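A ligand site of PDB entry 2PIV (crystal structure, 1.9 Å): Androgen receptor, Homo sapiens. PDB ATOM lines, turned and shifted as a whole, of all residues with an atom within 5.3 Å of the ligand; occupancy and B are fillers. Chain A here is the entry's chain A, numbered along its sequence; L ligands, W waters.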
ATOM      1  N   LEU A  33      13.001 -14.979 -33.439  1.00  0.00           N
ATOM      2  CA  LEU A  33      12.119 -14.118 -32.662  1.00  0.00           C
ATOM      3  C   LEU A  33      10.848 -13.772 -33.411  1.00  0.00           C
ATOM      4  O   LEU A  33       9.791 -13.584 -32.806  1.00  0.00           O
ATOM      5  CB  LEU A  33      12.868 -12.852 -32.246  1.00  0.00           C
ATOM      6  CG  LEU A  33      13.619 -12.918 -30.901  1.00  0.00           C
ATOM      7  CD1 LEU A  33      12.614 -13.059 -29.756  1.00  0.00           C
ATOM      8  CD2 LEU A  33      14.598 -14.094 -30.877  1.00  0.00           C
ATOM      9  N   LEU A  36       8.613 -16.601 -32.920  1.00  0.00           N
ATOM     10  CA  LEU A  36       8.148 -16.620 -31.535  1.00  0.00           C
ATOM     11  C   LEU A  36       7.013 -15.624 -31.350  1.00  0.00           C
ATOM     12  O   LEU A  36       6.057 -15.891 -30.605  1.00  0.00           O
ATOM     13  CB  LEU A  36       9.289 -16.274 -30.570  1.00  0.00           C
ATOM     14  CG  LEU A  36      10.195 -17.445 -30.173  1.00  0.00           C
ATOM     15  CD1 LEU A  36      11.322 -16.939 -29.294  1.00  0.00           C
ATOM     16  CD2 LEU A  36       9.350 -18.520 -29.414  1.00  0.00           C
ATOM     17  N   ASN A  37       7.091 -14.493 -32.056  1.00  0.00           N
ATOM     18  CA  ASN A  37       6.058 -13.479 -31.971  1.00  0.00           C
ATOM     19  C   ASN A  37       4.799 -13.969 -32.653  1.00  0.00           C
ATOM     20  O   ASN A  37       3.707 -13.804 -32.128  1.00  0.00           O
ATOM     21  CB  ASN A  37       6.500 -12.158 -32.607  1.00  0.00           C
ATOM     22  CG  ASN A  37       7.564 -11.446 -31.789  1.00  0.00           C
ATOM     23  OD1 ASN A  37       7.672 -11.663 -30.579  1.00  0.00           O
ATOM     24  ND2 ASN A  37       8.350 -10.574 -32.429  1.00  0.00           N
ATOM     25  N   LEU A  39       3.924 -16.941 -33.045  1.00  0.00           N
ATOM     26  CA  LEU A  39       3.405 -17.989 -32.177  1.00  0.00           C
ATOM     27  C   LEU A  39       2.631 -17.316 -31.023  1.00  0.00           C
ATOM     28  O   LEU A  39       1.568 -17.790 -30.616  1.00  0.00           O
ATOM     29  CB  LEU A  39       4.559 -18.814 -31.585  1.00  0.00           C
ATOM     30  CG  LEU A  39       4.149 -19.919 -30.605  1.00  0.00           C
ATOM     31  CD1 LEU A  39       3.216 -20.926 -31.295  1.00  0.00           C
ATOM     32  CD2 LEU A  39       5.382 -20.632 -30.088  1.00  0.00           C
ATOM     33  N   GLY A  40       3.180 -16.241 -30.481  1.00  0.00           N
ATOM     34  CA  GLY A  40       2.525 -15.537 -29.398  1.00  0.00           C
ATOM     35  C   GLY A  40       1.170 -15.022 -29.845  1.00  0.00           C
ATOM     36  O   GLY A  40       0.180 -15.101 -29.108  1.00  0.00           O
ATOM     37  N   GLN A  43      -1.182 -18.065 -30.152  1.00  0.00           N
ATOM     38  CA  GLN A  43      -1.528 -18.537 -28.823  1.00  0.00           C
ATOM     39  C   GLN A  43      -2.473 -17.581 -28.109  1.00  0.00           C
ATOM     40  O   GLN A  43      -3.325 -17.998 -27.329  1.00  0.00           O
ATOM     41  CB  GLN A  43      -0.252 -18.725 -27.989  1.00  0.00           C
ATOM     42  CG  GLN A  43       0.504 -20.014 -28.273  1.00  0.00           C
ATOM     43  CD  GLN A  43      -0.249 -21.252 -27.776  1.00  0.00           C
ATOM     44  OE1 GLN A  43       0.109 -22.384 -28.116  1.00  0.00           O
ATOM     45  NE2 GLN A  43      -1.283 -21.042 -26.960  1.00  0.00           N
ATOM     46  N   TRP A  73      -0.982 -13.064 -20.067  1.00  0.00           N
ATOM     47  CA  TRP A  73      -0.737 -13.968 -21.199  1.00  0.00           C
ATOM     48  C   TRP A  73       0.701 -14.520 -21.176  1.00  0.00           C
ATOM     49  O   TRP A  73       0.951 -15.686 -21.501  1.00  0.00           O
ATOM     50  CB  TRP A  73      -0.996 -13.254 -22.539  1.00  0.00           C
ATOM     51  CG  TRP A  73      -0.157 -12.028 -22.770  1.00  0.00           C
ATOM     52  CD1 TRP A  73      -0.415 -10.766 -22.348  1.00  0.00           C
ATOM     53  CD2 TRP A  73       1.114 -11.982 -23.463  1.00  0.00           C
ATOM     54  NE1 TRP A  73       0.603  -9.919 -22.743  1.00  0.00           N
ATOM     55  CE2 TRP A  73       1.532 -10.631 -23.432  1.00  0.00           C
ATOM     56  CE3 TRP A  73       1.901 -12.930 -24.115  1.00  0.00           C
ATOM     57  CZ2 TRP A  73       2.745 -10.228 -24.005  1.00  0.00           C
ATOM     58  CZ3 TRP A  73       3.084 -12.528 -24.691  1.00  0.00           C
ATOM     59  CH2 TRP A  73       3.497 -11.178 -24.647  1.00  0.00           C
ATOM     60  N   MET A  74       1.653 -13.682 -20.816  1.00  0.00           N
ATOM     61  CA  MET A  74       3.045 -14.131 -20.806  1.00  0.00           C
ATOM     62  C   MET A  74       3.254 -15.288 -19.837  1.00  0.00           C
ATOM     63  O   MET A  74       3.785 -16.325 -20.208  1.00  0.00           O
ATOM     64  CB  MET A  74       3.992 -12.983 -20.441  1.00  0.00           C
ATOM     65  CG  MET A  74       5.456 -13.347 -20.421  1.00  0.00           C
ATOM     66  SD  MET A  74       6.180 -13.697 -22.107  1.00  0.00           S
ATOM     67  CE  MET A  74       6.423 -11.953 -22.642  1.00  0.00           C
ATOM     68  N   MET A  77       1.431 -18.531 -21.005  1.00  0.00           N
ATOM     69  CA  MET A  77       2.090 -19.234 -22.102  1.00  0.00           C
ATOM     70  C   MET A  77       3.408 -19.915 -21.682  1.00  0.00           C
ATOM     71  O   MET A  77       3.678 -21.052 -22.096  1.00  0.00           O
ATOM     72  CB  MET A  77       2.364 -18.275 -23.252  1.00  0.00           C
ATOM     73  CG  MET A  77       1.078 -17.827 -23.975  1.00  0.00           C
ATOM     74  SD  MET A  77       1.372 -16.579 -25.196  1.00  0.00           S
ATOM     75  CE  MET A  77      -0.290 -16.068 -25.640  1.00  0.00           C
ATOM     76  N   VAL A  78       4.201 -19.222 -20.872  1.00  0.00           N
ATOM     77  CA  VAL A  78       5.463 -19.781 -20.385  1.00  0.00           C
ATOM     78  C   VAL A  78       5.201 -21.035 -19.549  1.00  0.00           C
ATOM     79  O   VAL A  78       5.911 -22.031 -19.686  1.00  0.00           O
ATOM     80  CB  VAL A  78       6.225 -18.754 -19.531  1.00  0.00           C
ATOM     81  CG1 VAL A  78       7.401 -19.413 -18.842  1.00  0.00           C
ATOM     82  CG2 VAL A  78       6.740 -17.618 -20.437  1.00  0.00           C
ATOM     83  N   MET A  81       4.078 -23.806 -21.826  1.00  0.00           N
ATOM     84  CA  MET A  81       5.220 -24.255 -22.607  1.00  0.00           C
ATOM     85  C   MET A  81       6.083 -25.170 -21.760  1.00  0.00           C
ATOM     86  O   MET A  81       6.551 -26.211 -22.227  1.00  0.00           O
ATOM     87  CB  MET A  81       6.026 -23.042 -23.089  1.00  0.00           C
ATOM     88  CG  MET A  81       7.183 -23.359 -24.025  1.00  0.00           C
ATOM     89  SD  MET A  81       8.719 -23.848 -23.202  1.00  0.00           S
ATOM     90  CE  MET A  81       9.173 -22.251 -22.411  1.00  0.00           C
ATOM     91  N   ARG A  84       4.512 -28.520 -21.653  1.00  0.00           N
ATOM     92  CA  ARG A  84       4.668 -29.214 -22.936  1.00  0.00           C
ATOM     93  C   ARG A  84       6.073 -29.810 -23.048  1.00  0.00           C
ATOM     94  O   ARG A  84       6.252 -30.984 -23.405  1.00  0.00           O
ATOM     95  CB  ARG A  84       4.452 -28.265 -24.114  1.00  0.00           C
ATOM     96  CG  ARG A  84       3.025 -27.916 -24.398  1.00  0.00           C
ATOM     97  CD  ARG A  84       2.921 -27.374 -25.838  1.00  0.00           C
ATOM     98  NE  ARG A  84       3.695 -26.157 -26.039  1.00  0.00           N
ATOM     99  CZ  ARG A  84       3.325 -24.960 -25.586  1.00  0.00           C
ATOM    100  NH1 ARG A  84       2.182 -24.832 -24.917  1.00  0.00           N
ATOM    101  NH2 ARG A  84       4.069 -23.895 -25.833  1.00  0.00           N
ATOM    102  N   PHE A  96       8.393 -24.916 -27.561  1.00  0.00           N
ATOM    103  CA  PHE A  96       7.489 -23.790 -27.811  1.00  0.00           C
ATOM    104  C   PHE A  96       6.356 -24.273 -28.698  1.00  0.00           C
ATOM    105  O   PHE A  96       5.182 -23.981 -28.449  1.00  0.00           O
ATOM    106  CB  PHE A  96       8.237 -22.642 -28.498  1.00  0.00           C
ATOM    107  CG  PHE A  96       9.236 -21.951 -27.621  1.00  0.00           C
ATOM    108  CD1 PHE A  96       8.813 -21.080 -26.602  1.00  0.00           C
ATOM    109  CD2 PHE A  96      10.595 -22.172 -27.794  1.00  0.00           C
ATOM    110  CE1 PHE A  96       9.726 -20.446 -25.774  1.00  0.00           C
ATOM    111  CE2 PHE A  96      11.540 -21.543 -26.956  1.00  0.00           C
ATOM    112  CZ  PHE A  96      11.094 -20.676 -25.945  1.00  0.00           C
ATOM    113  N   MET A 112      18.656 -14.730 -25.732  1.00  0.00           N
ATOM    114  CA  MET A 112      17.983 -14.754 -24.431  1.00  0.00           C
ATOM    115  C   MET A 112      18.229 -16.113 -23.783  1.00  0.00           C
ATOM    116  O   MET A 112      17.318 -16.753 -23.266  1.00  0.00           O
ATOM    117  CB  MET A 112      16.481 -14.494 -24.599  1.00  0.00           C
ATOM    118  CG  MET A 112      15.830 -15.364 -25.648  1.00  0.00           C
ATOM    119  SD  MET A 112      14.041 -14.949 -25.873  1.00  0.00           S
ATOM    120  CE  MET A 112      13.287 -16.297 -25.021  1.00  0.00           C
ATOM    121  N   MET A 119      13.451 -20.887 -17.904  1.00  0.00           N
ATOM    122  CA  MET A 119      12.239 -21.562 -18.363  1.00  0.00           C
ATOM    123  C   MET A 119      12.430 -23.092 -18.339  1.00  0.00           C
ATOM    124  O   MET A 119      11.516 -23.856 -18.074  1.00  0.00           O
ATOM    125  CB  MET A 119      11.879 -21.108 -19.776  1.00  0.00           C
ATOM    126  CG  MET A 119      11.531 -19.603 -19.839  1.00  0.00           C
ATOM    127  SD  MET A 119      10.615 -19.166 -21.323  1.00  0.00           S
ATOM    128  CE  MET A 119      11.870 -18.553 -22.386  1.00  0.00           C
ATOM    129  N   LEU A 205      10.873 -11.627 -19.437  1.00  0.00           N
ATOM    130  CA  LEU A 205      10.484 -11.727 -20.836  1.00  0.00           C
ATOM    131  C   LEU A 205       9.733 -10.467 -21.211  1.00  0.00           C
ATOM    132  O   LEU A 205       9.780 -10.026 -22.342  1.00  0.00           O
ATOM    133  CB  LEU A 205       9.616 -12.963 -21.086  1.00  0.00           C
ATOM    134  CG  LEU A 205      10.298 -14.316 -20.855  1.00  0.00           C
ATOM    135  CD1 LEU A 205       9.271 -15.437 -20.892  1.00  0.00           C
ATOM    136  CD2 LEU A 205      11.392 -14.538 -21.891  1.00  0.00           C
ATOM    137  N   PHE A 208      12.395  -7.963 -21.929  1.00  0.00           N
ATOM    138  CA  PHE A 208      13.074  -8.353 -23.154  1.00  0.00           C
ATOM    139  C   PHE A 208      12.258  -8.066 -24.411  1.00  0.00           C
ATOM    140  O   PHE A 208      12.756  -7.479 -25.380  1.00  0.00           O
ATOM    141  CB  PHE A 208      13.435  -9.843 -23.086  1.00  0.00           C
ATOM    142  CG  PHE A 208      14.265 -10.327 -24.241  1.00  0.00           C
ATOM    143  CD1 PHE A 208      13.663 -10.753 -25.426  1.00  0.00           C
ATOM    144  CD2 PHE A 208      15.660 -10.329 -24.158  1.00  0.00           C
ATOM    145  CE1 PHE A 208      14.438 -11.174 -26.504  1.00  0.00           C
ATOM    146  CE2 PHE A 208      16.454 -10.741 -25.236  1.00  0.00           C
ATOM    147  CZ  PHE A 208      15.838 -11.169 -26.419  1.00  0.00           C
ATOM    148  N   THR A 209      10.998  -8.486 -24.406  1.00  0.00           N
ATOM    149  CA  THR A 209      10.132  -8.259 -25.572  1.00  0.00           C
ATOM    150  C   THR A 209       9.885  -6.747 -25.781  1.00  0.00           C
ATOM    151  O   THR A 209       9.751  -6.244 -26.906  1.00  0.00           O
ATOM    152  CB  THR A 209       8.769  -8.993 -25.422  1.00  0.00           C
ATOM    153  OG1 THR A 209       8.119  -9.020 -26.690  1.00  0.00           O
ATOM    154  CG2 THR A 209       7.857  -8.274 -24.391  1.00  0.00           C
ATOM    155  N   LEU A 212      12.856  -5.276 -27.413  1.00  0.00           N
ATOM    156  CA  LEU A 212      12.926  -5.798 -28.761  1.00  0.00           C
ATOM    157  C   LEU A 212      11.963  -5.054 -29.694  1.00  0.00           C
ATOM    158  O   LEU A 212      12.287  -4.751 -30.829  1.00  0.00           O
ATOM    159  CB  LEU A 212      12.618  -7.298 -28.770  1.00  0.00           C
ATOM    160  CG  LEU A 212      12.722  -8.018 -30.118  1.00  0.00           C
ATOM    161  CD1 LEU A 212      14.101  -7.788 -30.705  1.00  0.00           C
ATOM    162  CD2 LEU A 212      12.462  -9.526 -29.895  1.00  0.00           C
ATOM    163  N   PHE A 223       6.668  -7.980 -35.508  1.00  0.00           N
ATOM    164  CA  PHE A 223       5.717  -8.108 -34.412  1.00  0.00           C
ATOM    165  C   PHE A 223       4.287  -8.024 -34.947  1.00  0.00           C
ATOM    166  O   PHE A 223       3.901  -7.014 -35.524  1.00  0.00           O
ATOM    167  CB  PHE A 223       5.910  -6.989 -33.371  1.00  0.00           C
ATOM    168  CG  PHE A 223       7.053  -7.231 -32.414  1.00  0.00           C
ATOM    169  CD1 PHE A 223       8.374  -7.035 -32.815  1.00  0.00           C
ATOM    170  CD2 PHE A 223       6.800  -7.647 -31.117  1.00  0.00           C
ATOM    171  CE1 PHE A 223       9.425  -7.241 -31.916  1.00  0.00           C
ATOM    172  CE2 PHE A 223       7.844  -7.860 -30.220  1.00  0.00           C
ATOM    173  CZ  PHE A 223       9.158  -7.660 -30.615  1.00  0.00           C
ATOM    174  N   ILE A 231       2.197  -5.194 -26.217  1.00  0.00           N
ATOM    175  CA  ILE A 231       3.527  -4.987 -25.658  1.00  0.00           C
ATOM    176  C   ILE A 231       3.888  -3.503 -25.513  1.00  0.00           C
ATOM    177  O   ILE A 231       4.744  -3.145 -24.707  1.00  0.00           O
ATOM    178  CB  ILE A 231       4.601  -5.689 -26.530  1.00  0.00           C
ATOM    179  CG1 ILE A 231       4.379  -7.202 -26.490  1.00  0.00           C
ATOM    180  CG2 ILE A 231       5.980  -5.310 -26.058  1.00  0.00           C
ATOM    181  CD1 ILE A 231       5.230  -7.969 -27.470  1.00  0.00           C
HETATM  182  C1  LIG L   1       5.255 -17.849 -27.174  1.00  0.00           C
HETATM  183  C2  LIG L   1       4.308 -18.939 -26.644  1.00  0.00           C
HETATM  184  C3  LIG L   1       5.184 -19.888 -25.737  1.00  0.00           C
HETATM  185  O1  LIG L   1       5.110 -21.066 -25.893  1.00  0.00           O
HETATM  186  C4  LIG L   1       6.052 -19.274 -24.716  1.00  0.00           C
HETATM  187  C5  LIG L   1       7.003 -18.182 -25.296  1.00  0.00           C
HETATM  188  C6  LIG L   1       7.926 -17.488 -24.212  1.00  0.00           C
HETATM  189  C7  LIG L   1       8.845 -16.464 -24.906  1.00  0.00           C
HETATM  190  C8  LIG L   1       8.063 -15.351 -25.693  1.00  0.00           C
HETATM  191  C9  LIG L   1       7.127 -16.049 -26.737  1.00  0.00           C
HETATM  192  C10 LIG L   1       6.114 -17.097 -26.091  1.00  0.00           C
HETATM  193  C11 LIG L   1       6.355 -14.906 -27.518  1.00  0.00           C
HETATM  194  C12 LIG L   1       7.232 -13.826 -28.183  1.00  0.00           C
HETATM  195  C13 LIG L   1       8.243 -13.218 -27.191  1.00  0.00           C
HETATM  196  C14 LIG L   1       8.998 -14.347 -26.407  1.00  0.00           C
HETATM  197  C15 LIG L   1       9.960 -13.551 -25.532  1.00  0.00           C
HETATM  198  C16 LIG L   1      10.481 -12.458 -26.522  1.00  0.00           C
HETATM  199  C17 LIG L   1       9.501 -12.524 -27.753  1.00  0.00           C
HETATM  200  O2  LIG L   1       9.244 -11.201 -28.244  1.00  0.00           O
HETATM  201  C18 LIG L   1       7.449 -12.244 -26.225  1.00  0.00           C
HETATM  202  C19 LIG L   1       5.160 -16.334 -25.077  1.00  0.00           C
HETATM  203  O   HOH W   1       2.366 -21.655 -24.418  1.00  0.00           O
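The backbone carbonyl oxygen (O) of Leu 33 lies close to the side-chain amide nitrogen (ND2) of Asn 37, at 3.4 Å.
The backbone carbonyl oxygen (O) of Phe 96 lies within hydrogen-bond range of the guanidinium group (NH2) of Arg 84 (2.8 Å).
Water W1 lies within hydrogen-bond range of the backbone carbonyl oxygen of Met 77, the guanidinium group of Arg 84 and an oxygen (O1) of the ligand.
Residues that only touch the ligand: Leu 33, Leu 36, Leu 39, Met 74, Met 77, Val 78, Met 81, Phe 96, Phe 208 and Leu 212.
13 residues have an atom within 4 Å of the ligand: Leu 33, Leu 36, Asn 37, Leu 39, Met 74, Met 77, Val 78, Met 81, Arg 84, Phe 96, Phe 208, Thr 209 and Leu 212.
Along chain A the residues within 4 Å of the ligand span positions 33 to 212.
The nearest printed residue that does not touch the ligand is Leu 205 (4.04 Å).
The side-chain amide oxygen of Asn 37 lies within hydrogen-bond range of an oxygen (O2) of the ligand.
The guanidinium group of Arg 84 lies within hydrogen-bond range of an oxygen (O1) of the ligand (3.0 Å).
An oxygen (O2) of the ligand lies within hydrogen-bond range of the side-chain hydroxyl of Thr 209.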
